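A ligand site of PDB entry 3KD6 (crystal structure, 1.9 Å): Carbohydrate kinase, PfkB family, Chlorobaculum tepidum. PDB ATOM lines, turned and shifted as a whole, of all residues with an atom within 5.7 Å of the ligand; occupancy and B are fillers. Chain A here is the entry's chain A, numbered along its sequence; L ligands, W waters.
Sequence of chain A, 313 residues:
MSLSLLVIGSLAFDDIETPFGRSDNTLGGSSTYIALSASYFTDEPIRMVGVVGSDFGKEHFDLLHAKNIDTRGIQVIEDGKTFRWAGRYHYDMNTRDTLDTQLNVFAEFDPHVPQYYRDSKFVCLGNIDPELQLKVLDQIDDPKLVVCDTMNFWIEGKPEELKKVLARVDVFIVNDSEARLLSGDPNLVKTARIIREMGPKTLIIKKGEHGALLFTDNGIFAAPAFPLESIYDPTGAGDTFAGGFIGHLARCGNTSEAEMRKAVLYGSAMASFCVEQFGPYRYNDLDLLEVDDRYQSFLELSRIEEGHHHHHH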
ATOM      1  N   SER A  10     -30.036  -8.106  26.575  1.00  0.00           N
ATOM      2  CA  SER A  10     -29.205  -7.648  27.670  1.00  0.00           C
ATOM      3  C   SER A  10     -28.169  -6.641  27.211  1.00  0.00           C
ATOM      4  O   SER A  10     -27.752  -6.613  26.059  1.00  0.00           O
ATOM      5  CB  SER A  10     -28.499  -8.838  28.344  1.00  0.00           C
ATOM      6  OG  SER A  10     -27.671  -9.548  27.432  1.00  0.00           O
ATOM      7  N   ALA A  12     -24.631  -5.376  28.936  1.00  0.00           N
ATOM      8  CA  ALA A  12     -23.824  -5.783  30.081  1.00  0.00           C
ATOM      9  C   ALA A  12     -22.327  -5.638  29.943  1.00  0.00           C
ATOM     10  O   ALA A  12     -21.811  -5.098  28.978  1.00  0.00           O
ATOM     11  CB  ALA A  12     -24.151  -7.215  30.418  1.00  0.00           C
ATOM     12  N   PHE A  13     -21.639  -6.146  30.964  1.00  0.00           N
ATOM     13  CA  PHE A  13     -20.190  -6.157  31.014  1.00  0.00           C
ATOM     14  C   PHE A  13     -19.798  -7.616  31.189  1.00  0.00           C
ATOM     15  O   PHE A  13     -20.319  -8.305  32.071  1.00  0.00           O
ATOM     16  CB  PHE A  13     -19.685  -5.323  32.197  1.00  0.00           C
ATOM     17  CG  PHE A  13     -19.881  -3.849  32.014  1.00  0.00           C
ATOM     18  CD1 PHE A  13     -19.242  -3.175  30.984  1.00  0.00           C
ATOM     19  CD2 PHE A  13     -20.713  -3.134  32.870  1.00  0.00           C
ATOM     20  CE1 PHE A  13     -19.433  -1.805  30.786  1.00  0.00           C
ATOM     21  CE2 PHE A  13     -20.917  -1.762  32.686  1.00  0.00           C
ATOM     22  CZ  PHE A  13     -20.274  -1.099  31.648  1.00  0.00           C
ATOM     23  N   ASP A  14     -18.891  -8.103  30.342  1.00  0.00           N
ATOM     24  CA  ASP A  14     -18.470  -9.491  30.422  1.00  0.00           C
ATOM     25  C   ASP A  14     -17.003  -9.685  30.775  1.00  0.00           C
ATOM     26  O   ASP A  14     -16.148  -8.918  30.339  1.00  0.00           O
ATOM     27  CB  ASP A  14     -18.698 -10.231  29.100  1.00  0.00           C
ATOM     28  CG  ASP A  14     -20.050  -9.991  28.490  1.00  0.00           C
ATOM     29  OD1 ASP A  14     -21.065  -9.966  29.225  1.00  0.00           O
ATOM     30  OD2 ASP A  14     -20.100  -9.848  27.247  1.00  0.00           O
ATOM     31  N   LEU A  27     -17.642  -4.477  27.263  1.00  0.00           N
ATOM     32  CA  LEU A  27     -19.001  -4.115  26.890  1.00  0.00           C
ATOM     33  C   LEU A  27     -19.609  -5.327  26.185  1.00  0.00           C
ATOM     34  O   LEU A  27     -18.960  -5.934  25.325  1.00  0.00           O
ATOM     35  CB  LEU A  27     -19.007  -2.917  25.938  1.00  0.00           C
ATOM     36  CG  LEU A  27     -20.338  -2.653  25.209  1.00  0.00           C
ATOM     37  CD1 LEU A  27     -21.416  -2.231  26.214  1.00  0.00           C
ATOM     38  CD2 LEU A  27     -20.141  -1.573  24.160  1.00  0.00           C
ATOM     39  N   GLY A  28     -20.833  -5.674  26.544  1.00  0.00           N
ATOM     40  CA  GLY A  28     -21.480  -6.818  25.924  1.00  0.00           C
ATOM     41  C   GLY A  28     -22.996  -6.779  26.064  1.00  0.00           C
ATOM     42  O   GLY A  28     -23.593  -5.695  26.144  1.00  0.00           O
ATOM     43  N   GLY A  29     -23.602  -7.960  26.100  1.00  0.00           N
ATOM     44  CA  GLY A  29     -25.047  -8.045  26.206  1.00  0.00           C
ATOM     45  C   GLY A  29     -25.599  -8.370  24.832  1.00  0.00           C
ATOM     46  O   GLY A  29     -25.096  -7.866  23.836  1.00  0.00           O
ATOM     47  N   SER A  30     -26.640  -9.204  24.788  1.00  0.00           N
ATOM     48  CA  SER A  30     -27.209  -9.603  23.494  1.00  0.00           C
ATOM     49  C   SER A  30     -27.742  -8.463  22.646  1.00  0.00           C
ATOM     50  O   SER A  30     -27.621  -8.498  21.423  1.00  0.00           O
ATOM     51  CB  SER A  30     -28.309 -10.667  23.696  1.00  0.00           C
ATOM     52  OG  SER A  30     -29.424 -10.182  24.417  1.00  0.00           O
ATOM     53  N   TYR A  33     -24.753  -6.534  20.799  1.00  0.00           N
ATOM     54  CA  TYR A  33     -24.270  -7.225  19.613  1.00  0.00           C
ATOM     55  C   TYR A  33     -25.293  -7.174  18.483  1.00  0.00           C
ATOM     56  O   TYR A  33     -24.948  -6.916  17.332  1.00  0.00           O
ATOM     57  CB  TYR A  33     -23.921  -8.674  19.976  1.00  0.00           C
ATOM     58  CG  TYR A  33     -22.575  -8.803  20.666  1.00  0.00           C
ATOM     59  CD1 TYR A  33     -21.400  -8.689  19.949  1.00  0.00           C
ATOM     60  CD2 TYR A  33     -22.489  -9.029  22.036  1.00  0.00           C
ATOM     61  CE1 TYR A  33     -20.162  -8.790  20.555  1.00  0.00           C
ATOM     62  CE2 TYR A  33     -21.247  -9.122  22.670  1.00  0.00           C
ATOM     63  CZ  TYR A  33     -20.083  -9.013  21.918  1.00  0.00           C
ATOM     64  OH  TYR A  33     -18.842  -9.103  22.509  1.00  0.00           O
ATOM     65  N   PHE A  83     -25.896  -5.406  34.251  1.00  0.00           N
ATOM     66  CA  PHE A  83     -25.902  -6.859  34.096  1.00  0.00           C
ATOM     67  C   PHE A  83     -24.448  -7.326  33.916  1.00  0.00           C
ATOM     68  O   PHE A  83     -23.681  -6.690  33.189  1.00  0.00           O
ATOM     69  CB  PHE A  83     -26.747  -7.209  32.861  1.00  0.00           C
ATOM     70  CG  PHE A  83     -26.931  -8.697  32.626  1.00  0.00           C
ATOM     71  CD1 PHE A  83     -28.214  -9.250  32.587  1.00  0.00           C
ATOM     72  CD2 PHE A  83     -25.840  -9.521  32.375  1.00  0.00           C
ATOM     73  CE1 PHE A  83     -28.399 -10.609  32.312  1.00  0.00           C
ATOM     74  CE2 PHE A  83     -26.016 -10.872  32.094  1.00  0.00           C
ATOM     75  CZ  PHE A  83     -27.295 -11.417  32.070  1.00  0.00           C
ATOM     76  N   TRP A  85     -21.700 -10.833  33.322  1.00  0.00           N
ATOM     77  CA  TRP A  85     -21.563 -12.216  32.889  1.00  0.00           C
ATOM     78  C   TRP A  85     -20.102 -12.614  32.743  1.00  0.00           C
ATOM     79  O   TRP A  85     -19.285 -11.805  32.319  1.00  0.00           O
ATOM     80  CB  TRP A  85     -22.284 -12.419  31.548  1.00  0.00           C
ATOM     81  CG  TRP A  85     -22.084 -13.778  30.965  1.00  0.00           C
ATOM     82  CD1 TRP A  85     -22.652 -14.944  31.377  1.00  0.00           C
ATOM     83  CD2 TRP A  85     -21.256 -14.117  29.836  1.00  0.00           C
ATOM     84  NE1 TRP A  85     -22.240 -15.987  30.584  1.00  0.00           N
ATOM     85  CE2 TRP A  85     -21.377 -15.501  29.635  1.00  0.00           C
ATOM     86  CE3 TRP A  85     -20.422 -13.378  28.987  1.00  0.00           C
ATOM     87  CZ2 TRP A  85     -20.698 -16.168  28.612  1.00  0.00           C
ATOM     88  CZ3 TRP A  85     -19.747 -14.034  27.973  1.00  0.00           C
ATOM     89  CH2 TRP A  85     -19.890 -15.423  27.793  1.00  0.00           C
ATOM     90  N   TYR A  89     -14.039 -20.078  27.395  1.00  0.00           N
ATOM     91  CA  TYR A  89     -13.962 -20.886  26.189  1.00  0.00           C
ATOM     92  C   TYR A  89     -12.790 -21.844  26.300  1.00  0.00           C
ATOM     93  O   TYR A  89     -11.958 -21.737  27.196  1.00  0.00           O
ATOM     94  CB  TYR A  89     -13.782 -19.997  24.962  1.00  0.00           C
ATOM     95  CG  TYR A  89     -14.945 -19.075  24.719  1.00  0.00           C
ATOM     96  CD1 TYR A  89     -16.040 -19.477  23.946  1.00  0.00           C
ATOM     97  CD2 TYR A  89     -14.976 -17.818  25.293  1.00  0.00           C
ATOM     98  CE1 TYR A  89     -17.133 -18.632  23.751  1.00  0.00           C
ATOM     99  CE2 TYR A  89     -16.072 -16.963  25.120  1.00  0.00           C
ATOM    100  CZ  TYR A  89     -17.144 -17.382  24.344  1.00  0.00           C
ATOM    101  OH  TYR A  89     -18.233 -16.530  24.178  1.00  0.00           O
ATOM    102  N   ARG A  96     -18.610 -23.033  25.569  1.00  0.00           N
ATOM    103  CA  ARG A  96     -18.137 -22.250  26.706  1.00  0.00           C
ATOM    104  C   ARG A  96     -18.879 -22.555  27.992  1.00  0.00           C
ATOM    105  O   ARG A  96     -19.981 -23.101  27.974  1.00  0.00           O
ATOM    106  CB  ARG A  96     -18.299 -20.757  26.403  1.00  0.00           C
ATOM    107  CG  ARG A  96     -19.750 -20.327  26.353  1.00  0.00           C
ATOM    108  CD  ARG A  96     -19.947 -18.921  25.810  1.00  0.00           C
ATOM    109  NE  ARG A  96     -21.358 -18.650  25.610  1.00  0.00           N
ATOM    110  CZ  ARG A  96     -21.842 -17.630  24.920  1.00  0.00           C
ATOM    111  NH1 ARG A  96     -21.023 -16.760  24.366  1.00  0.00           N
ATOM    112  NH2 ARG A  96     -23.157 -17.494  24.761  1.00  0.00           N
ATOM    113  N   THR A  98     -20.470 -20.928  31.512  1.00  0.00           N
ATOM    114  CA  THR A  98     -20.925 -19.681  32.111  1.00  0.00           C
ATOM    115  C   THR A  98     -20.418 -19.797  33.542  1.00  0.00           C
ATOM    116  O   THR A  98     -20.862 -20.667  34.285  1.00  0.00           O
ATOM    117  CB  THR A  98     -22.457 -19.565  32.116  1.00  0.00           C
ATOM    118  OG1 THR A  98     -22.917 -19.313  30.780  1.00  0.00           O
ATOM    119  CG2 THR A  98     -22.900 -18.427  33.025  1.00  0.00           C
ATOM    120  N   THR A 101     -23.420 -15.250  36.413  1.00  0.00           N
ATOM    121  CA  THR A 101     -24.505 -14.504  35.791  1.00  0.00           C
ATOM    122  C   THR A 101     -25.205 -13.698  36.875  1.00  0.00           C
ATOM    123  O   THR A 101     -25.822 -14.265  37.771  1.00  0.00           O
ATOM    124  CB  THR A 101     -25.533 -15.424  35.121  1.00  0.00           C
ATOM    125  OG1 THR A 101     -24.866 -16.305  34.209  1.00  0.00           O
ATOM    126  CG2 THR A 101     -26.561 -14.601  34.346  1.00  0.00           C
ATOM    127  N   ASN A 127     -31.767 -12.437  23.481  1.00  0.00           N
ATOM    128  CA  ASN A 127     -31.593 -13.222  24.687  1.00  0.00           C
ATOM    129  C   ASN A 127     -31.769 -12.387  25.950  1.00  0.00           C
ATOM    130  O   ASN A 127     -31.039 -11.419  26.168  1.00  0.00           O
ATOM    131  CB  ASN A 127     -30.198 -13.869  24.651  1.00  0.00           C
ATOM    132  CG  ASN A 127     -29.866 -14.612  25.918  1.00  0.00           C
ATOM    133  OD1 ASN A 127     -30.748 -15.147  26.594  1.00  0.00           O
ATOM    134  ND2 ASN A 127     -28.575 -14.667  26.240  1.00  0.00           N
ATOM    135  N   ILE A 128     -32.775 -12.767  26.730  1.00  0.00           N
ATOM    136  CA  ILE A 128     -33.131 -12.140  27.997  1.00  0.00           C
ATOM    137  C   ILE A 128     -34.296 -12.958  28.549  1.00  0.00           C
ATOM    138  O   ILE A 128     -34.881 -13.768  27.826  1.00  0.00           O
ATOM    139  CB  ILE A 128     -33.558 -10.648  27.812  1.00  0.00           C
ATOM    140  CG1 ILE A 128     -33.700  -9.967  29.174  1.00  0.00           C
ATOM    141  CG2 ILE A 128     -34.874 -10.558  27.089  1.00  0.00           C
ATOM    142  CD1 ILE A 128     -32.414  -9.895  29.947  1.00  0.00           C
ATOM    143  N   ASP A 129     -34.633 -12.766  29.822  1.00  0.00           N
ATOM    144  CA  ASP A 129     -35.730 -13.495  30.456  1.00  0.00           C
ATOM    145  C   ASP A 129     -36.962 -13.553  29.539  1.00  0.00           C
ATOM    146  O   ASP A 129     -37.454 -12.515  29.093  1.00  0.00           O
ATOM    147  CB  ASP A 129     -36.100 -12.806  31.779  1.00  0.00           C
ATOM    148  CG  ASP A 129     -37.161 -13.545  32.553  1.00  0.00           C
ATOM    149  OD1 ASP A 129     -38.246 -13.807  31.989  1.00  0.00           O
ATOM    150  OD2 ASP A 129     -36.921 -13.856  33.738  1.00  0.00           O
ATOM    151  N   MET A 151     -31.256 -18.690  25.550  1.00  0.00           N
ATOM    152  CA  MET A 151     -30.006 -19.187  26.093  1.00  0.00           C
ATOM    153  C   MET A 151     -30.303 -20.356  27.032  1.00  0.00           C
ATOM    154  O   MET A 151     -31.399 -20.441  27.585  1.00  0.00           O
ATOM    155  CB  MET A 151     -29.265 -18.081  26.841  1.00  0.00           C
ATOM    156  CG  MET A 151     -27.874 -18.478  27.287  1.00  0.00           C
ATOM    157  SD  MET A 151     -26.984 -17.098  28.271  1.00  0.00           S
ATOM    158  CE  MET A 151     -25.432 -16.911  27.132  1.00  0.00           C
ATOM    159  N   PHE A 153     -29.610 -20.848  29.909  1.00  0.00           N
ATOM    160  CA  PHE A 153     -30.036 -20.286  31.195  1.00  0.00           C
ATOM    161  C   PHE A 153     -31.556 -20.254  31.307  1.00  0.00           C
ATOM    162  O   PHE A 153     -32.127 -20.645  32.329  1.00  0.00           O
ATOM    163  CB  PHE A 153     -29.485 -18.859  31.331  1.00  0.00           C
ATOM    164  CG  PHE A 153     -29.611 -18.279  32.713  1.00  0.00           C
ATOM    165  CD1 PHE A 153     -28.662 -18.570  33.691  1.00  0.00           C
ATOM    166  CD2 PHE A 153     -30.654 -17.411  33.036  1.00  0.00           C
ATOM    167  CE1 PHE A 153     -28.738 -17.996  34.956  1.00  0.00           C
ATOM    168  CE2 PHE A 153     -30.744 -16.833  34.302  1.00  0.00           C
ATOM    169  CZ  PHE A 153     -29.782 -17.127  35.265  1.00  0.00           C
ATOM    170  N   TRP A 154     -32.206 -19.786  30.245  1.00  0.00           N
ATOM    171  CA  TRP A 154     -33.662 -19.681  30.225  1.00  0.00           C
ATOM    172  C   TRP A 154     -34.334 -20.977  29.799  1.00  0.00           C
ATOM    173  O   TRP A 154     -35.437 -21.283  30.241  1.00  0.00           O
ATOM    174  CB  TRP A 154     -34.088 -18.536  29.294  1.00  0.00           C
ATOM    175  CG  TRP A 154     -33.394 -17.238  29.605  1.00  0.00           C
ATOM    176  CD1 TRP A 154     -32.511 -16.570  28.812  1.00  0.00           C
ATOM    177  CD2 TRP A 154     -33.475 -16.492  30.821  1.00  0.00           C
ATOM    178  NE1 TRP A 154     -32.032 -15.450  29.451  1.00  0.00           N
ATOM    179  CE2 TRP A 154     -32.607 -15.385  30.703  1.00  0.00           C
ATOM    180  CE3 TRP A 154     -34.190 -16.664  32.024  1.00  0.00           C
ATOM    181  CZ2 TRP A 154     -32.442 -14.437  31.719  1.00  0.00           C
ATOM    182  CZ3 TRP A 154     -34.021 -15.727  33.031  1.00  0.00           C
ATOM    183  CH2 TRP A 154     -33.151 -14.628  32.878  1.00  0.00           C
ATOM    184  N   GLU A 178     -28.125 -25.518  22.130  1.00  0.00           N
ATOM    185  CA  GLU A 178     -29.411 -25.096  22.675  1.00  0.00           C
ATOM    186  C   GLU A 178     -30.518 -25.911  22.024  1.00  0.00           C
ATOM    187  O   GLU A 178     -31.439 -26.381  22.693  1.00  0.00           O
ATOM    188  CB  GLU A 178     -29.642 -23.595  22.418  1.00  0.00           C
ATOM    189  CG  GLU A 178     -28.565 -22.694  23.014  1.00  0.00           C
ATOM    190  CD  GLU A 178     -28.694 -21.234  22.586  1.00  0.00           C
ATOM    191  OE1 GLU A 178     -29.156 -20.964  21.457  1.00  0.00           O
ATOM    192  OE2 GLU A 178     -28.314 -20.336  23.382  1.00  0.00           O
ATOM    193  N   PRO A 234     -15.488 -15.989  20.452  1.00  0.00           N
ATOM    194  CA  PRO A 234     -16.836 -16.315  19.994  1.00  0.00           C
ATOM    195  C   PRO A 234     -17.950 -15.445  20.577  1.00  0.00           C
ATOM    196  O   PRO A 234     -19.042 -15.392  20.039  1.00  0.00           O
ATOM    197  CB  PRO A 234     -17.012 -17.777  20.400  1.00  0.00           C
ATOM    198  CG  PRO A 234     -15.589 -18.304  20.472  1.00  0.00           C
ATOM    199  CD  PRO A 234     -14.849 -17.148  21.103  1.00  0.00           C
ATOM    200  N   THR A 235     -17.661 -14.750  21.679  1.00  0.00           N
ATOM    201  CA  THR A 235     -18.675 -13.936  22.345  1.00  0.00           C
ATOM    202  C   THR A 235     -19.412 -12.988  21.397  1.00  0.00           C
ATOM    203  O   THR A 235     -18.786 -12.206  20.681  1.00  0.00           O
ATOM    204  CB  THR A 235     -18.060 -13.122  23.493  1.00  0.00           C
ATOM    205  OG1 THR A 235     -17.291 -13.988  24.332  1.00  0.00           O
ATOM    206  CG2 THR A 235     -19.156 -12.474  24.333  1.00  0.00           C
ATOM    207  N   GLY A 236     -20.740 -13.081  21.405  1.00  0.00           N
ATOM    208  CA  GLY A 236     -21.578 -12.228  20.589  1.00  0.00           C
ATOM    209  C   GLY A 236     -21.843 -12.698  19.169  1.00  0.00           C
ATOM    210  O   GLY A 236     -22.688 -12.124  18.480  1.00  0.00           O
ATOM    211  N   ALA A 237     -21.159 -13.754  18.733  1.00  0.00           N
ATOM    212  CA  ALA A 237     -21.313 -14.262  17.377  1.00  0.00           C
ATOM    213  C   ALA A 237     -22.769 -14.572  16.996  1.00  0.00           C
ATOM    214  O   ALA A 237     -23.240 -14.147  15.937  1.00  0.00           O
ATOM    215  CB  ALA A 237     -20.461 -15.511  17.201  1.00  0.00           C
ATOM    216  N   GLY A 238     -23.472 -15.299  17.862  1.00  0.00           N
ATOM    217  CA  GLY A 238     -24.852 -15.649  17.581  1.00  0.00           C
ATOM    218  C   GLY A 238     -25.792 -14.474  17.548  1.00  0.00           C
ATOM    219  O   GLY A 238     -26.783 -14.459  16.811  1.00  0.00           O
ATOM    220  N   ASP A 239     -25.497 -13.468  18.357  1.00  0.00           N
ATOM    221  CA  ASP A 239     -26.325 -12.279  18.392  1.00  0.00           C
ATOM    222  C   ASP A 239     -26.001 -11.344  17.240  1.00  0.00           C
ATOM    223  O   ASP A 239     -26.901 -10.671  16.724  1.00  0.00           O
ATOM    224  CB  ASP A 239     -26.216 -11.599  19.743  1.00  0.00           C
ATOM    225  CG  ASP A 239     -26.976 -12.366  20.820  1.00  0.00           C
ATOM    226  OD1 ASP A 239     -28.195 -12.572  20.637  1.00  0.00           O
ATOM    227  OD2 ASP A 239     -26.348 -12.771  21.825  1.00  0.00           O
ATOM    228  N   THR A 240     -24.737 -11.297  16.812  1.00  0.00           N
ATOM    229  CA  THR A 240     -24.413 -10.436  15.662  1.00  0.00           C
ATOM    230  C   THR A 240     -25.044 -11.113  14.433  1.00  0.00           C
ATOM    231  O   THR A 240     -25.407 -10.446  13.475  1.00  0.00           O
ATOM    232  CB  THR A 240     -22.884 -10.264  15.439  1.00  0.00           C
ATOM    233  OG1 THR A 240     -22.249 -11.535  15.320  1.00  0.00           O
ATOM    234  CG2 THR A 240     -22.257  -9.486  16.591  1.00  0.00           C
HETATM  235  P1  LIG L   1     -23.753 -14.840  22.585  1.00  0.00           P
HETATM  236  O1  LIG L   1     -24.249 -14.178  21.219  1.00  0.00           O
HETATM  237  O2  LIG L   1     -24.675 -16.083  22.920  1.00  0.00           O
HETATM  238  O3  LIG L   1     -22.240 -15.359  22.426  1.00  0.00           O
HETATM  239  O4  LIG L   1     -24.174 -13.969  23.470  1.00  0.00           O
HETATM  240  C1  LIG L   1     -23.104 -13.525  24.334  1.00  0.00           C
HETATM  241  C2  LIG L   1     -23.649 -12.443  25.299  1.00  0.00           C
HETATM  242  O5  LIG L   1     -24.854 -12.738  26.023  1.00  0.00           O
HETATM  243  C3  LIG L   1     -22.671 -11.805  26.339  1.00  0.00           C
HETATM  244  O6  LIG L   1     -22.096 -10.569  25.932  1.00  0.00           O
HETATM  245  C4  LIG L   1     -23.444 -11.674  27.661  1.00  0.00           C
HETATM  246  O7  LIG L   1     -23.545 -10.375  28.235  1.00  0.00           O
HETATM  247  C5  LIG L   1     -24.826 -12.200  27.359  1.00  0.00           C
HETATM  248  N1  LIG L   1     -25.422 -13.167  28.349  1.00  0.00           N
HETATM  249  C6  LIG L   1     -24.890 -14.165  29.103  1.00  0.00           C
HETATM  250  N2  LIG L   1     -25.855 -14.754  29.864  1.00  0.00           N
HETATM  251  C7  LIG L   1     -27.021 -14.113  29.605  1.00  0.00           C
HETATM  252  C8  LIG L   1     -28.444 -14.207  30.050  1.00  0.00           C
HETATM  253  N3  LIG L   1     -28.808 -15.144  30.955  1.00  0.00           N
HETATM  254  N4  LIG L   1     -29.361 -13.339  29.523  1.00  0.00           N
HETATM  255  C9  LIG L   1     -29.002 -12.390  28.612  1.00  0.00           C
HETATM  256  N5  LIG L   1     -27.731 -12.239  28.158  1.00  0.00           N
HETATM  257  C10 LIG L   1     -26.733 -13.063  28.614  1.00  0.00           C
HETATM  258  O   HOH W   1     -24.328 -18.827  20.981  1.00  0.00           O
HETATM  259  O   HOH W   2     -26.118 -16.701  31.767  1.00  0.00           O
HETATM  260  O   HOH W   3     -22.556 -16.772  20.036  1.00  0.00           O
HETATM  261  O   HOH W   4     -26.846 -13.907  24.224  1.00  0.00           O
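NH1 of Arg 96 is in hydrogen-bond range of OH of Tyr 89.
The backbone NH of Ser 30 sits at hydrogen-bond distance from the side-chain hydroxyl of Ser 10 (2.9 Å).
The backbone carbonyl oxygen of Gly 236 sits at hydrogen-bond distance from the side-chain hydroxyl of Thr 240 (3.2 Å).
OD1 of Asn 127 lies within hydrogen-bond range of NE1 of Trp 154, 3.1 Å away.
The backbone NH of Trp 85 is in hydrogen-bond range of the backbone carbonyl oxygen of Phe 13, at 3.1 Å.
The indole nitrogen (NE1) of Trp 85 sits at hydrogen-bond distance from the side-chain hydroxyl (OG1) of Thr 98.
N of Phe 13 is in hydrogen-bond range of O of Phe 83 (3.1 Å).
The side-chain hydroxyl (OG1) of Thr 235 lies within hydrogen-bond range of the side-chain hydroxyl (OH) of Tyr 89 (2.7 Å).
Ala 12 touches the ligand (CB to O7, 3.9 Å).
Gly 28 touches the ligand (CA to O6, 3.8 Å).
Tyr 33 touches the ligand.
Phe 83 touches the ligand (CZ to C8, 3.6 Å).
CD1 of Trp 85 touches C6 of the ligand (3.3 Å).
Phe 153 touches the ligand.
Pro 234 touches the ligand.
Thr 235 touches the ligand.
Ala 237 touches the ligand (N to O1, 3.99 Å).
Gly 238 touches the ligand.
Water W2 lies within hydrogen-bond range of N2 of the ligand, OG1 of Thr 101 and SD of Met 151.
Water W4 lies within hydrogen-bond range of OD2 of Asp 239 (2.7 Å), ND2 of Asn 127 (2.8 Å) and O4 of the ligand (2.8 Å).
Water W3 lies within hydrogen-bond range of N of Gly 238 (2.8 Å) and O3 of the ligand (2.8 Å).
OD2 of Asp 14 sits at hydrogen-bond distance from O6 of the ligand (2.5 Å).
The backbone NH (N) of Asp 239 sits at hydrogen-bond distance from an oxygen (O1) of the ligand (3.2 Å).
O1 of the ligand lies close to OD2 of Asp 239 (2.6 Å).
The guanidinium group (NH1) of Arg 96 is in salt-bridge range of an oxygen (O3) of the ligand (2.7 Å).
The side-chain hydroxyl (OG) of Ser 10 sits at hydrogen-bond distance from a nitrogen (N5) of the ligand (2.8 Å).
The backbone NH of Gly 236 is in hydrogen-bond range of an oxygen (O3) of the ligand (2.9 Å).
O6 of the ligand sits at hydrogen-bond distance from N of Gly 29 (3.0 Å).
The side-chain sulfur of Met 151 lies close to a nitrogen (N3) of the ligand (3.8 Å).
A nitrogen (N5) of the ligand is in hydrogen-bond range of the side-chain amide nitrogen (ND2) of Asn 127 (3.2 Å).
N4 of the ligand lies within hydrogen-bond range of NE1 of Trp 154 (3.4 Å).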
